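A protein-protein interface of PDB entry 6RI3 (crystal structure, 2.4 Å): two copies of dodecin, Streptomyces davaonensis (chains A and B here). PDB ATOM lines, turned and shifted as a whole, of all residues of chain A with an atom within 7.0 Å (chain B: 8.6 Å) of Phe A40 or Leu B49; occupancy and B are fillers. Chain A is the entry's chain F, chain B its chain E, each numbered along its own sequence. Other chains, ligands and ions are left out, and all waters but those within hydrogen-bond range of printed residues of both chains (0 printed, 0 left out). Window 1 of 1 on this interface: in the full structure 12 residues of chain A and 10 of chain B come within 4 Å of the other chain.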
ATOM      1  N   ILE A  23       5.703 -19.441  10.846  1.00  0.00           N
ATOM      2  CA  ILE A  23       5.262 -19.762   9.458  1.00  0.00           C
ATOM      3  C   ILE A  23       5.611 -21.227   9.176  1.00  0.00           C
ATOM      4  O   ILE A  23       4.709 -21.965   8.774  1.00  0.00           O
ATOM      5  CB  ILE A  23       5.882 -18.772   8.458  1.00  0.00           C
ATOM      6  CG1 ILE A  23       5.286 -17.374   8.637  1.00  0.00           C
ATOM      7  CG2 ILE A  23       5.748 -19.261   7.032  1.00  0.00           C
ATOM      8  CD1 ILE A  23       6.065 -16.266   7.924  1.00  0.00           C
ATOM      9  N   ILE A  27       2.989 -24.200   8.255  1.00  0.00           N
ATOM     10  CA  ILE A  27       3.062 -24.864   6.923  1.00  0.00           C
ATOM     11  C   ILE A  27       3.264 -26.370   7.123  1.00  0.00           C
ATOM     12  O   ILE A  27       2.519 -27.143   6.499  1.00  0.00           O
ATOM     13  CB  ILE A  27       4.177 -24.223   6.074  1.00  0.00           C
ATOM     14  CG1 ILE A  27       3.870 -22.749   5.794  1.00  0.00           C
ATOM     15  CG2 ILE A  27       4.436 -25.023   4.794  1.00  0.00           C
ATOM     16  CD1 ILE A  27       2.549 -22.505   5.127  1.00  0.00           C
ATOM     17  N   ASN A  36      -0.598 -31.077  -1.544  1.00  0.00           N
ATOM     18  CA  ASN A  36      -0.313 -30.254  -2.748  1.00  0.00           C
ATOM     19  C   ASN A  36      -0.282 -28.769  -2.377  1.00  0.00           C
ATOM     20  O   ASN A  36      -0.735 -27.948  -3.202  1.00  0.00           O
ATOM     21  CB  ASN A  36      -1.334 -30.515  -3.864  1.00  0.00           C
ATOM     22  CG  ASN A  36      -1.548 -31.987  -4.152  1.00  0.00           C
ATOM     23  OD1 ASN A  36      -0.606 -32.776  -4.084  1.00  0.00           O
ATOM     24  ND2 ASN A  36      -2.773 -32.352  -4.503  1.00  0.00           N
ATOM     25  N   LEU A  37       0.246 -28.424  -1.201  1.00  0.00           N
ATOM     26  CA  LEU A  37       0.478 -27.004  -0.821  1.00  0.00           C
ATOM     27  C   LEU A  37       1.347 -26.348  -1.902  1.00  0.00           C
ATOM     28  O   LEU A  37       2.413 -26.872  -2.205  1.00  0.00           O
ATOM     29  CB  LEU A  37       1.153 -26.909   0.547  1.00  0.00           C
ATOM     30  CG  LEU A  37       0.339 -27.381   1.753  1.00  0.00           C
ATOM     31  CD1 LEU A  37       0.966 -26.869   3.029  1.00  0.00           C
ATOM     32  CD2 LEU A  37      -1.106 -26.928   1.682  1.00  0.00           C
ATOM     33  N   ASP A  38       0.883 -25.231  -2.453  1.00  0.00           N
ATOM     34  CA  ASP A  38       1.526 -24.505  -3.571  1.00  0.00           C
ATOM     35  C   ASP A  38       2.119 -23.178  -3.063  1.00  0.00           C
ATOM     36  O   ASP A  38       3.247 -22.862  -3.444  1.00  0.00           O
ATOM     37  CB  ASP A  38       0.511 -24.285  -4.687  1.00  0.00           C
ATOM     38  CG  ASP A  38       1.165 -24.135  -6.051  1.00  0.00           C
ATOM     39  OD1 ASP A  38       1.554 -22.995  -6.438  1.00  0.00           O
ATOM     40  OD2 ASP A  38       1.260 -25.175  -6.734  1.00  0.00           O
ATOM     41  N   TRP A  39       1.376 -22.389  -2.284  1.00  0.00           N
ATOM     42  CA  TRP A  39       1.828 -21.036  -1.856  1.00  0.00           C
ATOM     43  C   TRP A  39       1.174 -20.636  -0.538  1.00  0.00           C
ATOM     44  O   TRP A  39       0.183 -21.277  -0.132  1.00  0.00           O
ATOM     45  CB  TRP A  39       1.541 -19.993  -2.943  1.00  0.00           C
ATOM     46  CG  TRP A  39       0.158 -19.437  -2.876  1.00  0.00           C
ATOM     47  CD1 TRP A  39      -0.288 -18.396  -2.109  1.00  0.00           C
ATOM     48  CD2 TRP A  39      -0.980 -19.918  -3.593  1.00  0.00           C
ATOM     49  NE1 TRP A  39      -1.627 -18.198  -2.306  1.00  0.00           N
ATOM     50  CE2 TRP A  39      -2.076 -19.105  -3.222  1.00  0.00           C
ATOM     51  CE3 TRP A  39      -1.178 -20.939  -4.525  1.00  0.00           C
ATOM     52  CZ2 TRP A  39      -3.354 -19.302  -3.740  1.00  0.00           C
ATOM     53  CZ3 TRP A  39      -2.440 -21.131  -5.040  1.00  0.00           C
ATOM     54  CH2 TRP A  39      -3.513 -20.331  -4.648  1.00  0.00           C
ATOM     55  N   PHE A  40       1.718 -19.598   0.091  1.00  0.00           N
ATOM     56  CA  PHE A  40       1.099 -18.932   1.258  1.00  0.00           C
ATOM     57  C   PHE A  40       1.304 -17.430   1.113  1.00  0.00           C
ATOM     58  O   PHE A  40       2.254 -17.019   0.440  1.00  0.00           O
ATOM     59  CB  PHE A  40       1.665 -19.469   2.576  1.00  0.00           C
ATOM     60  CG  PHE A  40       3.111 -19.126   2.808  1.00  0.00           C
ATOM     61  CD1 PHE A  40       3.461 -17.951   3.456  1.00  0.00           C
ATOM     62  CD2 PHE A  40       4.128 -19.941   2.323  1.00  0.00           C
ATOM     63  CE1 PHE A  40       4.797 -17.621   3.652  1.00  0.00           C
ATOM     64  CE2 PHE A  40       5.457 -19.604   2.531  1.00  0.00           C
ATOM     65  CZ  PHE A  40       5.789 -18.453   3.200  1.00  0.00           C
ATOM     66  N   GLU A  41       0.418 -16.658   1.740  1.00  0.00           N
ATOM     67  CA  GLU A  41       0.436 -15.184   1.800  1.00  0.00           C
ATOM     68  C   GLU A  41       0.246 -14.799   3.268  1.00  0.00           C
ATOM     69  O   GLU A  41      -0.788 -15.196   3.835  1.00  0.00           O
ATOM     70  CB  GLU A  41      -0.653 -14.621   0.873  1.00  0.00           C
ATOM     71  CG  GLU A  41      -0.637 -13.103   0.759  1.00  0.00           C
ATOM     72  CD  GLU A  41      -1.958 -12.453   0.389  1.00  0.00           C
ATOM     73  OE1 GLU A  41      -2.682 -13.048  -0.421  1.00  0.00           O
ATOM     74  OE2 GLU A  41      -2.238 -11.348   0.909  1.00  0.00           O
ATOM     75  N   VAL A  42       1.196 -14.089   3.878  1.00  0.00           N
ATOM     76  CA  VAL A  42       1.072 -13.632   5.291  1.00  0.00           C
ATOM     77  C   VAL A  42       0.011 -12.533   5.335  1.00  0.00           C
ATOM     78  O   VAL A  42       0.094 -11.606   4.545  1.00  0.00           O
ATOM     79  CB  VAL A  42       2.410 -13.151   5.863  1.00  0.00           C
ATOM     80  CG1 VAL A  42       2.261 -12.642   7.274  1.00  0.00           C
ATOM     81  CG2 VAL A  42       3.447 -14.260   5.827  1.00  0.00           C
ATOM     82  N   VAL A  59       1.178 -16.130  13.301  1.00  0.00           N
ATOM     83  CA  VAL A  59       1.164 -15.639  11.901  1.00  0.00           C
ATOM     84  C   VAL A  59      -0.008 -16.301  11.197  1.00  0.00           C
ATOM     85  O   VAL A  59      -0.028 -17.537  11.133  1.00  0.00           O
ATOM     86  CB  VAL A  59       2.500 -15.927  11.196  1.00  0.00           C
ATOM     87  CG1 VAL A  59       2.539 -15.328   9.791  1.00  0.00           C
ATOM     88  CG2 VAL A  59       3.673 -15.436  12.023  1.00  0.00           C
ATOM     89  N   MET A  61      -1.881 -16.911   7.695  1.00  0.00           N
ATOM     90  CA  MET A  61      -1.439 -17.074   6.291  1.00  0.00           C
ATOM     91  C   MET A  61      -2.640 -17.564   5.483  1.00  0.00           C
ATOM     92  O   MET A  61      -3.339 -18.461   5.967  1.00  0.00           O
ATOM     93  CB  MET A  61      -0.324 -18.118   6.181  1.00  0.00           C
ATOM     94  CG  MET A  61       0.900 -17.788   6.963  1.00  0.00           C
ATOM     95  SD  MET A  61       2.032 -19.203   6.924  1.00  0.00           S
ATOM     96  CE  MET A  61       1.332 -20.217   8.223  1.00  0.00           C
ATOM     97  N   LYS A  62      -2.859 -16.994   4.309  1.00  0.00           N
ATOM     98  CA  LYS A  62      -3.629 -17.648   3.233  1.00  0.00           C
ATOM     99  C   LYS A  62      -2.731 -18.770   2.727  1.00  0.00           C
ATOM    100  O   LYS A  62      -1.544 -18.500   2.507  1.00  0.00           O
ATOM    101  CB  LYS A  62      -4.029 -16.650   2.141  1.00  0.00           C
ATOM    102  CG  LYS A  62      -5.059 -15.613   2.558  1.00  0.00           C
ATOM    103  CD  LYS A  62      -5.682 -14.854   1.389  1.00  0.00           C
ATOM    104  CE  LYS A  62      -7.036 -14.264   1.717  1.00  0.00           C
ATOM    105  NZ  LYS A  62      -7.952 -15.284   2.303  1.00  0.00           N
ATOM    106  N   VAL A  63      -3.262 -19.986   2.607  1.00  0.00           N
ATOM    107  CA  VAL A  63      -2.508 -21.163   2.086  1.00  0.00           C
ATOM    108  C   VAL A  63      -3.298 -21.760   0.917  1.00  0.00           C
ATOM    109  O   VAL A  63      -4.475 -22.118   1.110  1.00  0.00           O
ATOM    110  CB  VAL A  63      -2.265 -22.195   3.199  1.00  0.00           C
ATOM    111  CG1 VAL A  63      -1.574 -23.446   2.672  1.00  0.00           C
ATOM    112  CG2 VAL A  63      -1.504 -21.570   4.364  1.00  0.00           C
ATOM    113  N   GLY A  64      -2.679 -21.799  -0.261  1.00  0.00           N
ATOM    114  CA  GLY A  64      -3.248 -22.354  -1.494  1.00  0.00           C
ATOM    115  C   GLY A  64      -2.719 -23.751  -1.748  1.00  0.00           C
ATOM    116  O   GLY A  64      -1.530 -23.990  -1.541  1.00  0.00           O
ATOM    117  N   VAL B  19      12.708 -13.786   4.649  1.00  0.00           N
ATOM    118  CA  VAL B  19      12.080 -12.458   4.389  1.00  0.00           C
ATOM    119  C   VAL B  19      13.197 -11.415   4.280  1.00  0.00           C
ATOM    120  O   VAL B  19      13.217 -10.662   3.283  1.00  0.00           O
ATOM    121  CB  VAL B  19      11.058 -12.129   5.492  1.00  0.00           C
ATOM    122  CG1 VAL B  19      10.588 -10.681   5.446  1.00  0.00           C
ATOM    123  CG2 VAL B  19       9.876 -13.093   5.434  1.00  0.00           C
ATOM    124  N   GLU B  44       3.700  -6.925   1.277  1.00  0.00           N
ATOM    125  CA  GLU B  44       3.226  -8.318   1.129  1.00  0.00           C
ATOM    126  C   GLU B  44       4.400  -9.270   1.333  1.00  0.00           C
ATOM    127  O   GLU B  44       5.493  -8.991   0.808  1.00  0.00           O
ATOM    128  CB  GLU B  44       2.544  -8.503  -0.228  1.00  0.00           C
ATOM    129  CG  GLU B  44       1.975  -9.900  -0.427  1.00  0.00           C
ATOM    130  CD  GLU B  44       1.267 -10.142  -1.746  1.00  0.00           C
ATOM    131  OE1 GLU B  44       0.269  -9.455  -2.000  1.00  0.00           O
ATOM    132  OE2 GLU B  44       1.742 -11.025  -2.507  1.00  0.00           O
ATOM    133  N   VAL B  45       4.163 -10.362   2.055  1.00  0.00           N
ATOM    134  CA  VAL B  45       5.121 -11.489   2.175  1.00  0.00           C
ATOM    135  C   VAL B  45       4.405 -12.772   1.735  1.00  0.00           C
ATOM    136  O   VAL B  45       3.360 -13.111   2.327  1.00  0.00           O
ATOM    137  CB  VAL B  45       5.663 -11.586   3.609  1.00  0.00           C
ATOM    138  CG1 VAL B  45       6.649 -12.728   3.726  1.00  0.00           C
ATOM    139  CG2 VAL B  45       6.300 -10.298   4.099  1.00  0.00           C
ATOM    140  N   ARG B  46       4.949 -13.429   0.714  1.00  0.00           N
ATOM    141  CA  ARG B  46       4.427 -14.661   0.096  1.00  0.00           C
ATOM    142  C   ARG B  46       5.524 -15.730   0.120  1.00  0.00           C
ATOM    143  O   ARG B  46       6.723 -15.374   0.246  1.00  0.00           O
ATOM    144  CB  ARG B  46       4.028 -14.402  -1.360  1.00  0.00           C
ATOM    145  CG  ARG B  46       2.567 -14.048  -1.550  1.00  0.00           C
ATOM    146  CD  ARG B  46       2.164 -14.077  -3.019  1.00  0.00           C
ATOM    147  NE  ARG B  46       1.031 -13.191  -3.254  1.00  0.00           N
ATOM    148  CZ  ARG B  46      -0.258 -13.536  -3.220  1.00  0.00           C
ATOM    149  NH1 ARG B  46      -0.612 -14.785  -2.966  1.00  0.00           N
ATOM    150  NH2 ARG B  46      -1.188 -12.618  -3.434  1.00  0.00           N
ATOM    151  N   GLY B  47       5.129 -16.978  -0.109  1.00  0.00           N
ATOM    152  CA  GLY B  47       6.057 -18.098  -0.291  1.00  0.00           C
ATOM    153  C   GLY B  47       5.576 -19.016  -1.386  1.00  0.00           C
ATOM    154  O   GLY B  47       4.363 -19.218  -1.517  1.00  0.00           O
ATOM    155  N   GLN B  48       6.516 -19.568  -2.145  1.00  0.00           N
ATOM    156  CA  GLN B  48       6.302 -20.746  -3.016  1.00  0.00           C
ATOM    157  C   GLN B  48       6.602 -21.975  -2.161  1.00  0.00           C
ATOM    158  O   GLN B  48       7.670 -21.990  -1.512  1.00  0.00           O
ATOM    159  CB  GLN B  48       7.163 -20.613  -4.274  1.00  0.00           C
ATOM    160  CG  GLN B  48       6.401 -20.160  -5.528  1.00  0.00           C
ATOM    161  CD  GLN B  48       5.489 -21.242  -6.074  1.00  0.00           C
ATOM    162  OE1 GLN B  48       5.792 -22.433  -6.034  1.00  0.00           O
ATOM    163  NE2 GLN B  48       4.330 -20.841  -6.581  1.00  0.00           N
ATOM    164  N   LEU B  49       5.671 -22.914  -2.073  1.00  0.00           N
ATOM    165  CA  LEU B  49       5.871 -24.192  -1.342  1.00  0.00           C
ATOM    166  C   LEU B  49       6.172 -25.278  -2.365  1.00  0.00           C
ATOM    167  O   LEU B  49       5.641 -25.230  -3.467  1.00  0.00           O
ATOM    168  CB  LEU B  49       4.630 -24.520  -0.507  1.00  0.00           C
ATOM    169  CG  LEU B  49       4.275 -23.459   0.529  1.00  0.00           C
ATOM    170  CD1 LEU B  49       2.875 -23.691   1.072  1.00  0.00           C
ATOM    171  CD2 LEU B  49       5.292 -23.464   1.669  1.00  0.00           C
ATOM    172  N   ASN B  50       7.017 -26.232  -1.976  1.00  0.00           N
ATOM    173  CA  ASN B  50       7.330 -27.474  -2.725  1.00  0.00           C
ATOM    174  C   ASN B  50       7.351 -28.622  -1.701  1.00  0.00           C
ATOM    175  O   ASN B  50       8.029 -28.499  -0.711  1.00  0.00           O
ATOM    176  CB  ASN B  50       8.600 -27.253  -3.528  1.00  0.00           C
ATOM    177  CG  ASN B  50       9.318 -28.502  -3.998  1.00  0.00           C
ATOM    178  OD1 ASN B  50       8.718 -29.514  -4.365  1.00  0.00           O
ATOM    179  ND2 ASN B  50      10.623 -28.439  -3.899  1.00  0.00           N
ATOM    180  N   ASP B  51       6.535 -29.651  -1.944  1.00  0.00           N
ATOM    181  CA  ASP B  51       6.020 -30.589  -0.904  1.00  0.00           C
ATOM    182  C   ASP B  51       5.362 -29.706   0.159  1.00  0.00           C
ATOM    183  O   ASP B  51       4.488 -28.924  -0.234  1.00  0.00           O
ATOM    184  CB  ASP B  51       7.144 -31.490  -0.380  1.00  0.00           C
ATOM    185  CG  ASP B  51       7.874 -32.293  -1.449  1.00  0.00           C
ATOM    186  OD1 ASP B  51       7.224 -32.694  -2.439  1.00  0.00           O
ATOM    187  OD2 ASP B  51       9.094 -32.529  -1.277  1.00  0.00           O
ATOM    188  N   GLY B  52       5.800 -29.787   1.411  1.00  0.00           N
ATOM    189  CA  GLY B  52       5.395 -28.872   2.506  1.00  0.00           C
ATOM    190  C   GLY B  52       6.571 -28.017   2.971  1.00  0.00           C
ATOM    191  O   GLY B  52       6.676 -27.751   4.223  1.00  0.00           O
ATOM    192  N   GLN B  53       7.468 -27.648   2.042  1.00  0.00           N
ATOM    193  CA  GLN B  53       8.713 -26.879   2.356  1.00  0.00           C
ATOM    194  C   GLN B  53       8.708 -25.551   1.587  1.00  0.00           C
ATOM    195  O   GLN B  53       8.223 -25.487   0.445  1.00  0.00           O
ATOM    196  CB  GLN B  53       9.984 -27.641   2.001  1.00  0.00           C
ATOM    197  CG  GLN B  53      10.490 -28.597   3.075  1.00  0.00           C
ATOM    198  CD  GLN B  53      11.931 -28.300   3.414  1.00  0.00           C
ATOM    199  OE1 GLN B  53      12.326 -28.272   4.585  1.00  0.00           O
ATOM    200  NE2 GLN B  53      12.730 -28.047   2.384  1.00  0.00           N
ATOM    201  N   ILE B  54       9.177 -24.515   2.269  1.00  0.00           N
ATOM    202  CA  ILE B  54       9.222 -23.129   1.741  1.00  0.00           C
ATOM    203  C   ILE B  54      10.431 -23.029   0.821  1.00  0.00           C
ATOM    204  O   ILE B  54      11.542 -23.030   1.335  1.00  0.00           O
ATOM    205  CB  ILE B  54       9.255 -22.113   2.897  1.00  0.00           C
ATOM    206  CG1 ILE B  54       8.083 -22.311   3.867  1.00  0.00           C
ATOM    207  CG2 ILE B  54       9.273 -20.701   2.350  1.00  0.00           C
ATOM    208  CD1 ILE B  54       8.296 -21.696   5.218  1.00  0.00           C
ATOM    209  N   ALA B  55      10.206 -22.938  -0.486  1.00  0.00           N
ATOM    210  CA  ALA B  55      11.259 -22.930  -1.533  1.00  0.00           C
ATOM    211  C   ALA B  55      11.733 -21.501  -1.814  1.00  0.00           C
ATOM    212  O   ALA B  55      12.948 -21.312  -1.933  1.00  0.00           O
ATOM    213  CB  ALA B  55      10.753 -23.576  -2.798  1.00  0.00           C
ATOM    214  N   HIS B  56      10.804 -20.551  -1.928  1.00  0.00           N
ATOM    215  CA  HIS B  56      11.083 -19.123  -2.223  1.00  0.00           C
ATOM    216  C   HIS B  56      10.248 -18.251  -1.289  1.00  0.00           C
ATOM    217  O   HIS B  56       9.037 -18.537  -1.161  1.00  0.00           O
ATOM    218  CB  HIS B  56      10.795 -18.790  -3.698  1.00  0.00           C
ATOM    219  CG  HIS B  56      11.994 -18.811  -4.571  1.00  0.00           C
ATOM    220  ND1 HIS B  56      12.230 -19.837  -5.464  1.00  0.00           N
ATOM    221  CD2 HIS B  56      13.024 -17.942  -4.699  1.00  0.00           C
ATOM    222  CE1 HIS B  56      13.359 -19.598  -6.110  1.00  0.00           C
ATOM    223  NE2 HIS B  56      13.866 -18.440  -5.657  1.00  0.00           N
ATOM    224  N   TRP B  57      10.865 -17.201  -0.749  1.00  0.00           N
ATOM    225  CA  TRP B  57      10.159 -16.060  -0.114  1.00  0.00           C
ATOM    226  C   TRP B  57      10.076 -14.910  -1.123  1.00  0.00           C
ATOM    227  O   TRP B  57      11.056 -14.721  -1.859  1.00  0.00           O
ATOM    228  CB  TRP B  57      10.894 -15.621   1.136  1.00  0.00           C
ATOM    229  CG  TRP B  57      10.991 -16.653   2.205  1.00  0.00           C
ATOM    230  CD1 TRP B  57      11.885 -17.677   2.272  1.00  0.00           C
ATOM    231  CD2 TRP B  57      10.172 -16.752   3.384  1.00  0.00           C
ATOM    232  NE1 TRP B  57      11.683 -18.403   3.421  1.00  0.00           N
ATOM    233  CE2 TRP B  57      10.648 -17.859   4.125  1.00  0.00           C
ATOM    234  CE3 TRP B  57       9.059 -16.052   3.869  1.00  0.00           C
ATOM    235  CZ2 TRP B  57      10.061 -18.263   5.321  1.00  0.00           C
ATOM    236  CZ3 TRP B  57       8.496 -16.440   5.063  1.00  0.00           C
ATOM    237  CH2 TRP B  57       8.976 -17.542   5.771  1.00  0.00           C
ATOM    238  N   GLN B  58       8.898 -14.297  -1.244  1.00  0.00           N
ATOM    239  CA  GLN B  58       8.641 -13.136  -2.143  1.00  0.00           C
ATOM    240  C   GLN B  58       8.101 -12.003  -1.288  1.00  0.00           C
ATOM    241  O   GLN B  58       7.036 -12.160  -0.675  1.00  0.00           O
ATOM    242  CB  GLN B  58       7.627 -13.430  -3.243  1.00  0.00           C
ATOM    243  CG  GLN B  58       8.007 -14.591  -4.146  1.00  0.00           C
ATOM    244  CD  GLN B  58       6.877 -14.948  -5.074  1.00  0.00           C
ATOM    245  OE1 GLN B  58       5.900 -14.207  -5.214  1.00  0.00           O
ATOM    246  NE2 GLN B  58       7.016 -16.097  -5.717  1.00  0.00           N
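Of the 16 printed residues of chain B, 9 touch a printed residue of chain A. Printed residues of chain A that touch a printed residue of chain B: Ile A23, Ile A27, Leu A37, Asp A38, Trp A39, Phe A40, Glu A41 and Val A42. Hydrophobic or aromatic side chains of chain A that line the printed part of chain B: Ile A23, Ile A27, Leu A37, Trp A39, Phe A40 and Val A42.
The backbone carbonyl oxygen of Val B45 is in hydrogen-bond range of the backbone NH of Val A42 (2.8 Å). The guanidinium group (NH2) of Arg B46 lies within salt-bridge range of the side-chain carboxylate (OE1) of Glu A41, 3.4 Å away. The backbone carbonyl oxygen of Phe A40 sits at hydrogen-bond distance from the backbone NH of Gly B47 (2.9 Å). The backbone NH (N) of Leu B49 is in hydrogen-bond range of the backbone carbonyl oxygen (O) of Asp A38, 2.8 Å away.
No position is printed for both chains. Of the 19 pairs that touch across the chains among the printed residues, none has its exchanged pair printed and touching as well.
The guanidinium group (NH2) of Arg B46 is in salt-bridge range of the side-chain carboxylate (OE2) of Glu B44. The backbone NH (N) of Arg B46 sits at hydrogen-bond distance from the backbone carbonyl oxygen (O) of Gln B58 (2.8 Å). The backbone NH (N) of Gln B48 lies within hydrogen-bond range of the backbone carbonyl oxygen (O) of His B56 (2.9 Å). N of Asp A38 is in hydrogen-bond range of O of Gly A64 (2.9 Å). The backbone carbonyl oxygen (O) of Trp A39 sits at hydrogen-bond distance from the backbone NH (N) of Gly A64, at 2.9 Å. O of Glu A41 lies within hydrogen-bond range of N of Lys A62 (2.8 Å).
Among the printed residues, pairs that only touch across the chains: Ile A23 with Ile B54, Ile A23 with Trp B57, Ile A27 with Leu B49, Ile A27 with Gly B52, Leu A37 with Leu B49, Leu A37 with Asp B51, Asp A38 with Gln B48, Trp A39 with Arg B46, Trp A39 with Gly B47, Trp A39 with Leu B49, Phe A40 with Arg B46, Phe A40 with Leu B49, Phe A40 with Ile B54, Phe A40 with Trp B57 and Glu A41 with Val B45.
Phe A40 touches just these residues of chain B: Arg B46 (3.2 Å), Gly B47 (2.9 Å), Leu B49 (3.8 Å), Ile B54 (3.97 Å) and Trp B57 (3.9 Å). Printed residues of chain B within 4 Å of Glu A41: Val B45 (3.6 Å) and Arg B46 (3.4 Å). Val B19 touches none of the printed residues of chain A. Of the printed residues of chain A, Arg B46 touches Trp A39, Phe A40 and Glu A41. Leu B49 touches just these residues of chain A: Ile A27, Leu A37, Asp A38, Trp A39 and Phe A40. The nearest residue of chain A that does not touch Leu B49 is Val A63 (4.7 Å). The nearest printed residue of chain B that does not touch Glu A41 is Glu B44 (4.3 Å).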
